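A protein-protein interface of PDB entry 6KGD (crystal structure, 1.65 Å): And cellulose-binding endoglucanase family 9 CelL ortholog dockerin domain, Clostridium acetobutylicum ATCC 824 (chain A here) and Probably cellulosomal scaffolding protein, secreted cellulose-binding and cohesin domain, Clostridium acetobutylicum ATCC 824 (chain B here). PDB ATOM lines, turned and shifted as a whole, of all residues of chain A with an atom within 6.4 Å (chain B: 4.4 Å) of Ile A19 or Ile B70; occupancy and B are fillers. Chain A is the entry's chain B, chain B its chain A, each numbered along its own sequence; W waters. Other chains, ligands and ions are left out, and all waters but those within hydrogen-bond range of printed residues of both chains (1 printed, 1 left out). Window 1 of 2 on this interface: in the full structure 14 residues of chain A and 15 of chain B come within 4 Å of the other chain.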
ATOM      1  N   GLY A   6     -16.930   6.360  -4.380  1.00  0.00           N
ATOM      2  CA  GLY A   6     -16.753   6.048  -5.795  1.00  0.00           C
ATOM      3  C   GLY A   6     -16.765   7.246  -6.734  1.00  0.00           C
ATOM      4  O   GLY A   6     -17.085   7.128  -7.921  1.00  0.00           O
ATOM      5  N   LEU A   8     -14.759   9.126  -8.659  1.00  0.00           N
ATOM      6  CA  LEU A   8     -13.397   8.974  -9.134  1.00  0.00           C
ATOM      7  C   LEU A   8     -12.890  10.246  -9.799  1.00  0.00           C
ATOM      8  O   LEU A   8     -11.683  10.500  -9.816  1.00  0.00           O
ATOM      9  CB  LEU A   8     -13.305   7.805 -10.107  1.00  0.00           C
ATOM     10  CG  LEU A   8     -13.770   6.416  -9.641  1.00  0.00           C
ATOM     11  CD1 LEU A   8     -13.246   5.379 -10.646  1.00  0.00           C
ATOM     12  CD2 LEU A   8     -13.359   6.082  -8.240  1.00  0.00           C
ATOM     13  N   ASN A  15     -21.799   8.740 -10.634  1.00  0.00           N
ATOM     14  CA  ASN A  15     -22.651   8.509 -11.781  1.00  0.00           C
ATOM     15  C   ASN A  15     -21.854   7.791 -12.858  1.00  0.00           C
ATOM     16  O   ASN A  15     -20.767   7.271 -12.616  1.00  0.00           O
ATOM     17  CB  ASN A  15     -23.257   9.823 -12.295  1.00  0.00           C
ATOM     18  CG  ASN A  15     -22.236  10.797 -12.855  1.00  0.00           C
ATOM     19  OD1 ASN A  15     -21.101  10.444 -13.195  1.00  0.00           O
ATOM     20  ND2 ASN A  15     -22.644  12.054 -12.965  1.00  0.00           N
ATOM     21  N   GLY A  16     -22.423   7.720 -14.048  1.00  0.00           N
ATOM     22  CA  GLY A  16     -21.821   6.932 -15.103  1.00  0.00           C
ATOM     23  C   GLY A  16     -20.435   7.387 -15.521  1.00  0.00           C
ATOM     24  O   GLY A  16     -19.649   6.579 -16.017  1.00  0.00           O
ATOM     25  N   ARG A  17     -20.104   8.667 -15.333  1.00  0.00           N
ATOM     26  CA  ARG A  17     -18.739   9.095 -15.632  1.00  0.00           C
ATOM     27  C   ARG A  17     -17.735   8.335 -14.777  1.00  0.00           C
ATOM     28  O   ARG A  17     -16.654   7.967 -15.251  1.00  0.00           O
ATOM     29  CB  ARG A  17     -18.577  10.590 -15.408  1.00  0.00           C
ATOM     30  CG  ARG A  17     -19.423  11.483 -16.278  1.00  0.00           C
ATOM     31  CD  ARG A  17     -18.966  12.911 -16.069  1.00  0.00           C
ATOM     32  NE  ARG A  17     -19.757  13.962 -16.694  1.00  0.00           N
ATOM     33  CZ  ARG A  17     -19.693  14.307 -17.970  1.00  0.00           C
ATOM     34  NH1 ARG A  17     -18.930  13.628 -18.816  1.00  0.00           N
ATOM     35  NH2 ARG A  17     -20.421  15.334 -18.409  1.00  0.00           N
ATOM     36  N   ASP A  18     -18.072   8.106 -13.512  1.00  0.00           N
ATOM     37  CA  ASP A  18     -17.192   7.369 -12.615  1.00  0.00           C
ATOM     38  C   ASP A  18     -17.059   5.919 -13.035  1.00  0.00           C
ATOM     39  O   ASP A  18     -15.976   5.327 -12.910  1.00  0.00           O
ATOM     40  CB  ASP A  18     -17.726   7.473 -11.191  1.00  0.00           C
ATOM     41  CG  ASP A  18     -17.828   8.906 -10.731  1.00  0.00           C
ATOM     42  OD1 ASP A  18     -16.784   9.583 -10.626  1.00  0.00           O
ATOM     43  OD2 ASP A  18     -18.949   9.373 -10.508  1.00  0.00           O
ATOM     44  N   ILE A  19     -18.150   5.314 -13.522  1.00  0.00           N
ATOM     45  CA  ILE A  19     -18.065   3.943 -14.026  1.00  0.00           C
ATOM     46  C   ILE A  19     -17.112   3.854 -15.209  1.00  0.00           C
ATOM     47  O   ILE A  19     -16.287   2.935 -15.300  1.00  0.00           O
ATOM     48  CB  ILE A  19     -19.466   3.426 -14.388  1.00  0.00           C
ATOM     49  CG1 ILE A  19     -20.322   3.329 -13.131  1.00  0.00           C
ATOM     50  CG2 ILE A  19     -19.368   2.079 -15.093  1.00  0.00           C
ATOM     51  CD1 ILE A  19     -21.774   2.925 -13.398  1.00  0.00           C
ATOM     52  N   VAL A  20     -17.235   4.768 -16.164  1.00  0.00           N
ATOM     53  CA  VAL A  20     -16.335   4.734 -17.311  1.00  0.00           C
ATOM     54  C   VAL A  20     -14.888   4.824 -16.857  1.00  0.00           C
ATOM     55  O   VAL A  20     -14.029   4.076 -17.336  1.00  0.00           O
ATOM     56  CB  VAL A  20     -16.672   5.862 -18.294  1.00  0.00           C
ATOM     57  CG1 VAL A  20     -15.631   5.942 -19.382  1.00  0.00           C
ATOM     58  CG2 VAL A  20     -18.040   5.631 -18.881  1.00  0.00           C
ATOM     59  N   MET A  21     -14.596   5.721 -15.916  1.00  0.00           N
ATOM     60  CA  MET A  21     -13.215   5.889 -15.479  1.00  0.00           C
ATOM     61  C   MET A  21     -12.697   4.648 -14.773  1.00  0.00           C
ATOM     62  O   MET A  21     -11.549   4.246 -14.987  1.00  0.00           O
ATOM     63  CB  MET A  21     -13.083   7.107 -14.579  1.00  0.00           C
ATOM     64  CG  MET A  21     -13.296   8.382 -15.351  1.00  0.00           C
ATOM     65  SD  MET A  21     -13.121   9.786 -14.250  1.00  0.00           S
ATOM     66  CE  MET A  21     -11.404   9.655 -13.794  1.00  0.00           C
ATOM     67  N   MET A  22     -13.544   4.000 -13.963  1.00  0.00           N
ATOM     68  CA  MET A  22     -13.145   2.748 -13.337  1.00  0.00           C
ATOM     69  C   MET A  22     -12.871   1.676 -14.384  1.00  0.00           C
ATOM     70  O   MET A  22     -11.901   0.915 -14.272  1.00  0.00           O
ATOM     71  CB  MET A  22     -14.214   2.280 -12.374  1.00  0.00           C
ATOM     72  CG  MET A  22     -13.937   0.910 -11.748  1.00  0.00           C
ATOM     73  SD  MET A  22     -12.576   0.918 -10.565  1.00  0.00           S
ATOM     74  CE  MET A  22     -13.450   1.450  -9.086  1.00  0.00           C
ATOM     75  N   ARG A  23     -13.748   1.568 -15.387  1.00  0.00           N
ATOM     76  CA  ARG A  23     -13.499   0.587 -16.435  1.00  0.00           C
ATOM     77  C   ARG A  23     -12.219   0.901 -17.194  1.00  0.00           C
ATOM     78  O   ARG A  23     -11.473  -0.017 -17.559  1.00  0.00           O
ATOM     79  CB  ARG A  23     -14.685   0.489 -17.384  1.00  0.00           C
ATOM     80  CG  ARG A  23     -15.885  -0.179 -16.749  1.00  0.00           C
ATOM     81  CD  ARG A  23     -16.748  -0.821 -17.808  1.00  0.00           C
ATOM     82  NE  ARG A  23     -17.984  -1.367 -17.264  1.00  0.00           N
ATOM     83  CZ  ARG A  23     -19.181  -0.827 -17.439  1.00  0.00           C
ATOM     84  NH1 ARG A  23     -19.319   0.280 -18.131  1.00  0.00           N
ATOM     85  NH2 ARG A  23     -20.247  -1.407 -16.914  1.00  0.00           N
ATOM     86  N   GLN A  24     -11.939   2.188 -17.436  1.00  0.00           N
ATOM     87  CA  GLN A  24     -10.699   2.543 -18.123  1.00  0.00           C
ATOM     88  C   GLN A  24      -9.488   2.127 -17.292  1.00  0.00           C
ATOM     89  O   GLN A  24      -8.544   1.534 -17.815  1.00  0.00           O
ATOM     90  CB  GLN A  24     -10.664   4.035 -18.429  1.00  0.00           C
ATOM     91  CG  GLN A  24     -11.655   4.454 -19.520  1.00  0.00           C
ATOM     92  CD  GLN A  24     -11.755   5.952 -19.616  1.00  0.00           C
ATOM     93  OE1 GLN A  24     -11.644   6.652 -18.607  1.00  0.00           O
ATOM     94  NE2 GLN A  24     -11.918   6.462 -20.831  1.00  0.00           N
ATOM     95  N   LEU A  52     -15.490  -2.185  -8.997  1.00  0.00           N
ATOM     96  CA  LEU A  52     -16.399  -1.821 -10.069  1.00  0.00           C
ATOM     97  C   LEU A  52     -17.811  -2.246  -9.721  1.00  0.00           C
ATOM     98  O   LEU A  52     -18.762  -1.480  -9.915  1.00  0.00           O
ATOM     99  CB  LEU A  52     -15.943  -2.445 -11.378  1.00  0.00           C
ATOM    100  CG  LEU A  52     -16.906  -2.238 -12.551  1.00  0.00           C
ATOM    101  CD1 LEU A  52     -17.150  -0.780 -12.901  1.00  0.00           C
ATOM    102  CD2 LEU A  52     -16.372  -2.989 -13.759  1.00  0.00           C
ATOM    103  N   LEU A  55     -19.368   0.083  -7.280  1.00  0.00           N
ATOM    104  CA  LEU A  55     -19.707   1.349  -7.903  1.00  0.00           C
ATOM    105  C   LEU A  55     -21.005   1.235  -8.684  1.00  0.00           C
ATOM    106  O   LEU A  55     -21.885   2.097  -8.575  1.00  0.00           O
ATOM    107  CB  LEU A  55     -18.543   1.767  -8.802  1.00  0.00           C
ATOM    108  CG  LEU A  55     -18.725   3.019  -9.650  1.00  0.00           C
ATOM    109  CD1 LEU A  55     -19.126   4.196  -8.789  1.00  0.00           C
ATOM    110  CD2 LEU A  55     -17.435   3.292 -10.405  1.00  0.00           C
ATOM    111  N   ILE A  56     -21.141   0.158  -9.450  1.00  0.00           N
ATOM    112  CA  ILE A  56     -22.367  -0.085 -10.200  1.00  0.00           C
ATOM    113  C   ILE A  56     -23.557  -0.143  -9.257  1.00  0.00           C
ATOM    114  O   ILE A  56     -24.617   0.437  -9.530  1.00  0.00           O
ATOM    115  CB  ILE A  56     -22.235  -1.365 -11.035  1.00  0.00           C
ATOM    116  CG1 ILE A  56     -21.317  -1.119 -12.237  1.00  0.00           C
ATOM    117  CG2 ILE A  56     -23.611  -1.871 -11.486  1.00  0.00           C
ATOM    118  CD1 ILE A  56     -20.738  -2.387 -12.853  1.00  0.00           C
ATOM    119  N   VAL A  59     -24.533   3.408  -8.231  1.00  0.00           N
ATOM    120  CA  VAL A  59     -25.290   4.066  -9.291  1.00  0.00           C
ATOM    121  C   VAL A  59     -26.683   3.458  -9.425  1.00  0.00           C
ATOM    122  O   VAL A  59     -27.667   4.181  -9.654  1.00  0.00           O
ATOM    123  CB  VAL A  59     -24.492   4.008 -10.603  1.00  0.00           C
ATOM    124  CG1 VAL A  59     -25.313   4.543 -11.765  1.00  0.00           C
ATOM    125  CG2 VAL A  59     -23.186   4.788 -10.474  1.00  0.00           C
ATOM    126  N   SER A  60     -26.801   2.137  -9.278  1.00  0.00           N
ATOM    127  CA  SER A  60     -28.077   1.451  -9.485  1.00  0.00           C
ATOM    128  C   SER A  60     -29.070   1.675  -8.349  1.00  0.00           C
ATOM    129  O   SER A  60     -30.285   1.623  -8.583  1.00  0.00           O
ATOM    130  CB  SER A  60     -27.804  -0.038  -9.670  1.00  0.00           C
ATOM    131  OG  SER A  60     -28.978  -0.791  -9.919  1.00  0.00           O
ATOM    132  N   ASN A  61     -28.591   1.954  -7.140  1.00  0.00           N
ATOM    133  CA  ASN A  61     -29.453   1.838  -5.967  1.00  0.00           C
ATOM    134  C   ASN A  61     -29.517   3.064  -5.079  1.00  0.00           C
ATOM    135  O   ASN A  61     -30.507   3.256  -4.360  1.00  0.00           O
ATOM    136  CB  ASN A  61     -29.001   0.650  -5.097  1.00  0.00           C
ATOM    137  CG  ASN A  61     -29.272  -0.664  -5.738  1.00  0.00           C
ATOM    138  OD1 ASN A  61     -30.427  -1.034  -5.928  1.00  0.00           O
ATOM    139  ND2 ASN A  61     -28.216  -1.394  -6.077  1.00  0.00           N
ATOM    140  N   TYR B  67     -23.368  -5.073 -17.425  1.00  0.00           N
ATOM    141  CA  TYR B  67     -23.848  -3.838 -16.810  1.00  0.00           C
ATOM    142  C   TYR B  67     -23.670  -2.640 -17.736  1.00  0.00           C
ATOM    143  O   TYR B  67     -23.342  -1.548 -17.297  1.00  0.00           O
ATOM    144  CB  TYR B  67     -23.187  -3.600 -15.446  1.00  0.00           C
ATOM    145  CG  TYR B  67     -23.385  -4.807 -14.555  1.00  0.00           C
ATOM    146  CD1 TYR B  67     -24.581  -5.003 -13.895  1.00  0.00           C
ATOM    147  CD2 TYR B  67     -22.401  -5.772 -14.437  1.00  0.00           C
ATOM    148  CE1 TYR B  67     -24.780  -6.128 -13.109  1.00  0.00           C
ATOM    149  CE2 TYR B  67     -22.597  -6.898 -13.660  1.00  0.00           C
ATOM    150  CZ  TYR B  67     -23.777  -7.065 -13.002  1.00  0.00           C
ATOM    151  OH  TYR B  67     -23.944  -8.188 -12.227  1.00  0.00           O
ATOM    152  N   SER B  68     -23.960  -2.843 -19.019  1.00  0.00           N
ATOM    153  CA  SER B  68     -24.065  -1.741 -19.963  1.00  0.00           C
ATOM    154  C   SER B  68     -25.284  -0.871 -19.725  1.00  0.00           C
ATOM    155  O   SER B  68     -25.342   0.255 -20.236  1.00  0.00           O
ATOM    156  CB  SER B  68     -24.122  -2.294 -21.385  1.00  0.00           C
ATOM    157  OG  SER B  68     -25.310  -3.065 -21.555  1.00  0.00           O
ATOM    158  N   PHE B  69     -26.264  -1.360 -18.978  1.00  0.00           N
ATOM    159  CA  PHE B  69     -27.538  -0.664 -18.841  1.00  0.00           C
ATOM    160  C   PHE B  69     -27.949  -0.747 -17.383  1.00  0.00           C
ATOM    161  O   PHE B  69     -28.347  -1.818 -16.894  1.00  0.00           O
ATOM    162  CB  PHE B  69     -28.573  -1.286 -19.768  1.00  0.00           C
ATOM    163  CG  PHE B  69     -29.832  -0.471 -19.915  1.00  0.00           C
ATOM    164  CD1 PHE B  69     -29.834   0.654 -20.703  1.00  0.00           C
ATOM    165  CD2 PHE B  69     -30.999  -0.858 -19.278  1.00  0.00           C
ATOM    166  CE1 PHE B  69     -30.995   1.406 -20.866  1.00  0.00           C
ATOM    167  CE2 PHE B  69     -32.155  -0.108 -19.429  1.00  0.00           C
ATOM    168  CZ  PHE B  69     -32.149   1.011 -20.232  1.00  0.00           C
ATOM    169  N   ILE B  70     -27.852   0.375 -16.689  1.00  0.00           N
ATOM    170  CA  ILE B  70     -28.113   0.453 -15.255  1.00  0.00           C
ATOM    171  C   ILE B  70     -29.296   1.382 -15.053  1.00  0.00           C
ATOM    172  O   ILE B  70     -29.312   2.494 -15.595  1.00  0.00           O
ATOM    173  CB  ILE B  70     -26.895   0.968 -14.468  1.00  0.00           C
ATOM    174  CG1 ILE B  70     -25.717  -0.020 -14.560  1.00  0.00           C
ATOM    175  CG2 ILE B  70     -27.247   1.230 -13.011  1.00  0.00           C
ATOM    176  CD1 ILE B  70     -24.363   0.665 -14.311  1.00  0.00           C
ATOM    177  N   VAL B  71     -30.278   0.917 -14.279  1.00  0.00           N
ATOM    178  CA  VAL B  71     -31.489   1.668 -13.992  1.00  0.00           C
ATOM    179  C   VAL B  71     -31.613   1.862 -12.487  1.00  0.00           C
ATOM    180  O   VAL B  71     -31.530   0.903 -11.708  1.00  0.00           O
ATOM    181  CB  VAL B  71     -32.734   0.965 -14.547  1.00  0.00           C
ATOM    182  CG1 VAL B  71     -33.974   1.808 -14.272  1.00  0.00           C
ATOM    183  CG2 VAL B  71     -32.578   0.724 -16.030  1.00  0.00           C
ATOM    184  N   ASN B  72     -31.863   3.093 -12.090  1.00  0.00           N
ATOM    185  CA  ASN B  72     -32.087   3.451 -10.696  1.00  0.00           C
ATOM    186  C   ASN B  72     -33.510   3.974 -10.587  1.00  0.00           C
ATOM    187  O   ASN B  72     -33.821   5.069 -11.085  1.00  0.00           O
ATOM    188  CB  ASN B  72     -31.075   4.500 -10.233  1.00  0.00           C
ATOM    189  CG  ASN B  72     -31.165   4.774  -8.762  1.00  0.00           C
ATOM    190  OD1 ASN B  72     -32.244   4.839  -8.202  1.00  0.00           O
ATOM    191  ND2 ASN B  72     -30.010   4.948  -8.118  1.00  0.00           N
ATOM    192  N   SER B  80     -33.537   6.986 -13.338  1.00  0.00           N
ATOM    193  CA  SER B  80     -32.201   7.325 -13.827  1.00  0.00           C
ATOM    194  C   SER B  80     -31.684   6.147 -14.641  1.00  0.00           C
ATOM    195  O   SER B  80     -31.635   5.016 -14.134  1.00  0.00           O
ATOM    196  CB  SER B  80     -31.256   7.640 -12.676  1.00  0.00           C
ATOM    197  OG  SER B  80     -31.705   8.787 -11.968  1.00  0.00           O
ATOM    198  N   ILE B  81     -31.329   6.411 -15.897  1.00  0.00           N
ATOM    199  CA  ILE B  81     -30.807   5.415 -16.832  1.00  0.00           C
ATOM    200  C   ILE B  81     -29.357   5.765 -17.153  1.00  0.00           C
ATOM    201  O   ILE B  81     -29.042   6.914 -17.486  1.00  0.00           O
ATOM    202  CB  ILE B  81     -31.642   5.363 -18.123  1.00  0.00           C
ATOM    203  CG1 ILE B  81     -33.088   4.958 -17.813  1.00  0.00           C
ATOM    204  CG2 ILE B  81     -30.989   4.400 -19.137  1.00  0.00           C
ATOM    205  CD1 ILE B  81     -34.037   5.098 -19.014  1.00  0.00           C
ATOM    206  N   THR B  82     -28.472   4.775 -17.029  1.00  0.00           N
ATOM    207  CA  THR B  82     -27.056   4.908 -17.367  1.00  0.00           C
ATOM    208  C   THR B  82     -26.693   3.833 -18.390  1.00  0.00           C
ATOM    209  O   THR B  82     -26.776   2.645 -18.104  1.00  0.00           O
ATOM    210  CB  THR B  82     -26.187   4.802 -16.117  1.00  0.00           C
ATOM    211  OG1 THR B  82     -26.588   5.816 -15.175  1.00  0.00           O
ATOM    212  CG2 THR B  82     -24.713   5.017 -16.454  1.00  0.00           C
HETATM  213  O   HOH W   1     -25.324   7.825 -13.977  1.00  0.00           O
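O of Ile B70 sits at hydrogen-bond distance from N of Thr B82, at 2.8 Å.
The backbone NH (N) of Asn B72 lies within hydrogen-bond range of the backbone carbonyl oxygen (O) of Ser B80 (2.8 Å).
The backbone carbonyl oxygen (O) of Tyr B67 is in hydrogen-bond range of the guanidinium group (NH2) of Arg A23.
The backbone carbonyl oxygen (O) of Val A59 sits at hydrogen-bond distance from the side-chain amide nitrogen (ND2) of Asn B72, at 2.9 Å.
O of Ser A60 sits close to ND2 of Asn B72 (3.4 Å).
N of Asn A61 sits close to ND2 of Asn B72 (3.5 Å).
O of Val B71 sits close to O of Ser A60.
Among the printed residues, no Asp or Glu carboxylate lies within 4 Å of a Lys or Arg side-chain nitrogen of the other chain.
CG2 of Thr B82 touches CA of Gly A16, at 3.7 Å.
Ile B70 touches Ile A19.
CB of Tyr B67 touches CD1 of Ile A56, at 3.8 Å.
Ile A56 touches Ile B70 (CG2 to CD1, 3.9 Å).
Val A59 touches Thr B82 (CG1 to OG1, 3.9 Å).
Ser A60 touches Ile B70.
Water W1 lies within hydrogen-bond range of the side-chain hydroxyl (OG1) of Thr B82 (2.7 Å) and the backbone NH (N) of Gly A16 (2.9 Å).
Ile A19 touches one residue of chain B.
Of chain A, only Ile A19 (3.6 Å), Ile A56 (3.9 Å) and Ser A60 (3.6 Å) come within 4 Å of Ile B70.
Printed residues of chain B within 4 Å of Ser A60: Ile B70, Val B71 and Asn B72.
Printed residues of chain B within 4 Å of Arg A23: Tyr B67.
Printed residues of chain A within 4 Å of Asn B72: Val A59, Ser A60 and Asn A61.
Printed residues of chain B within 4 Å of Val A59: Asn B72 and Thr B82.
Printed residues of chain A within 4 Å of Thr B82: Gly A16 (3.7 Å) and Val A59 (3.9 Å).
Leu A52 touches none of the printed residues of chain B.
The nearest residue of chain A that does not touch Ile B70 is Val A59 (4.03 Å).
The nearest printed residue of chain B that does not touch Asn A61 is Val B71 (5.5 Å).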
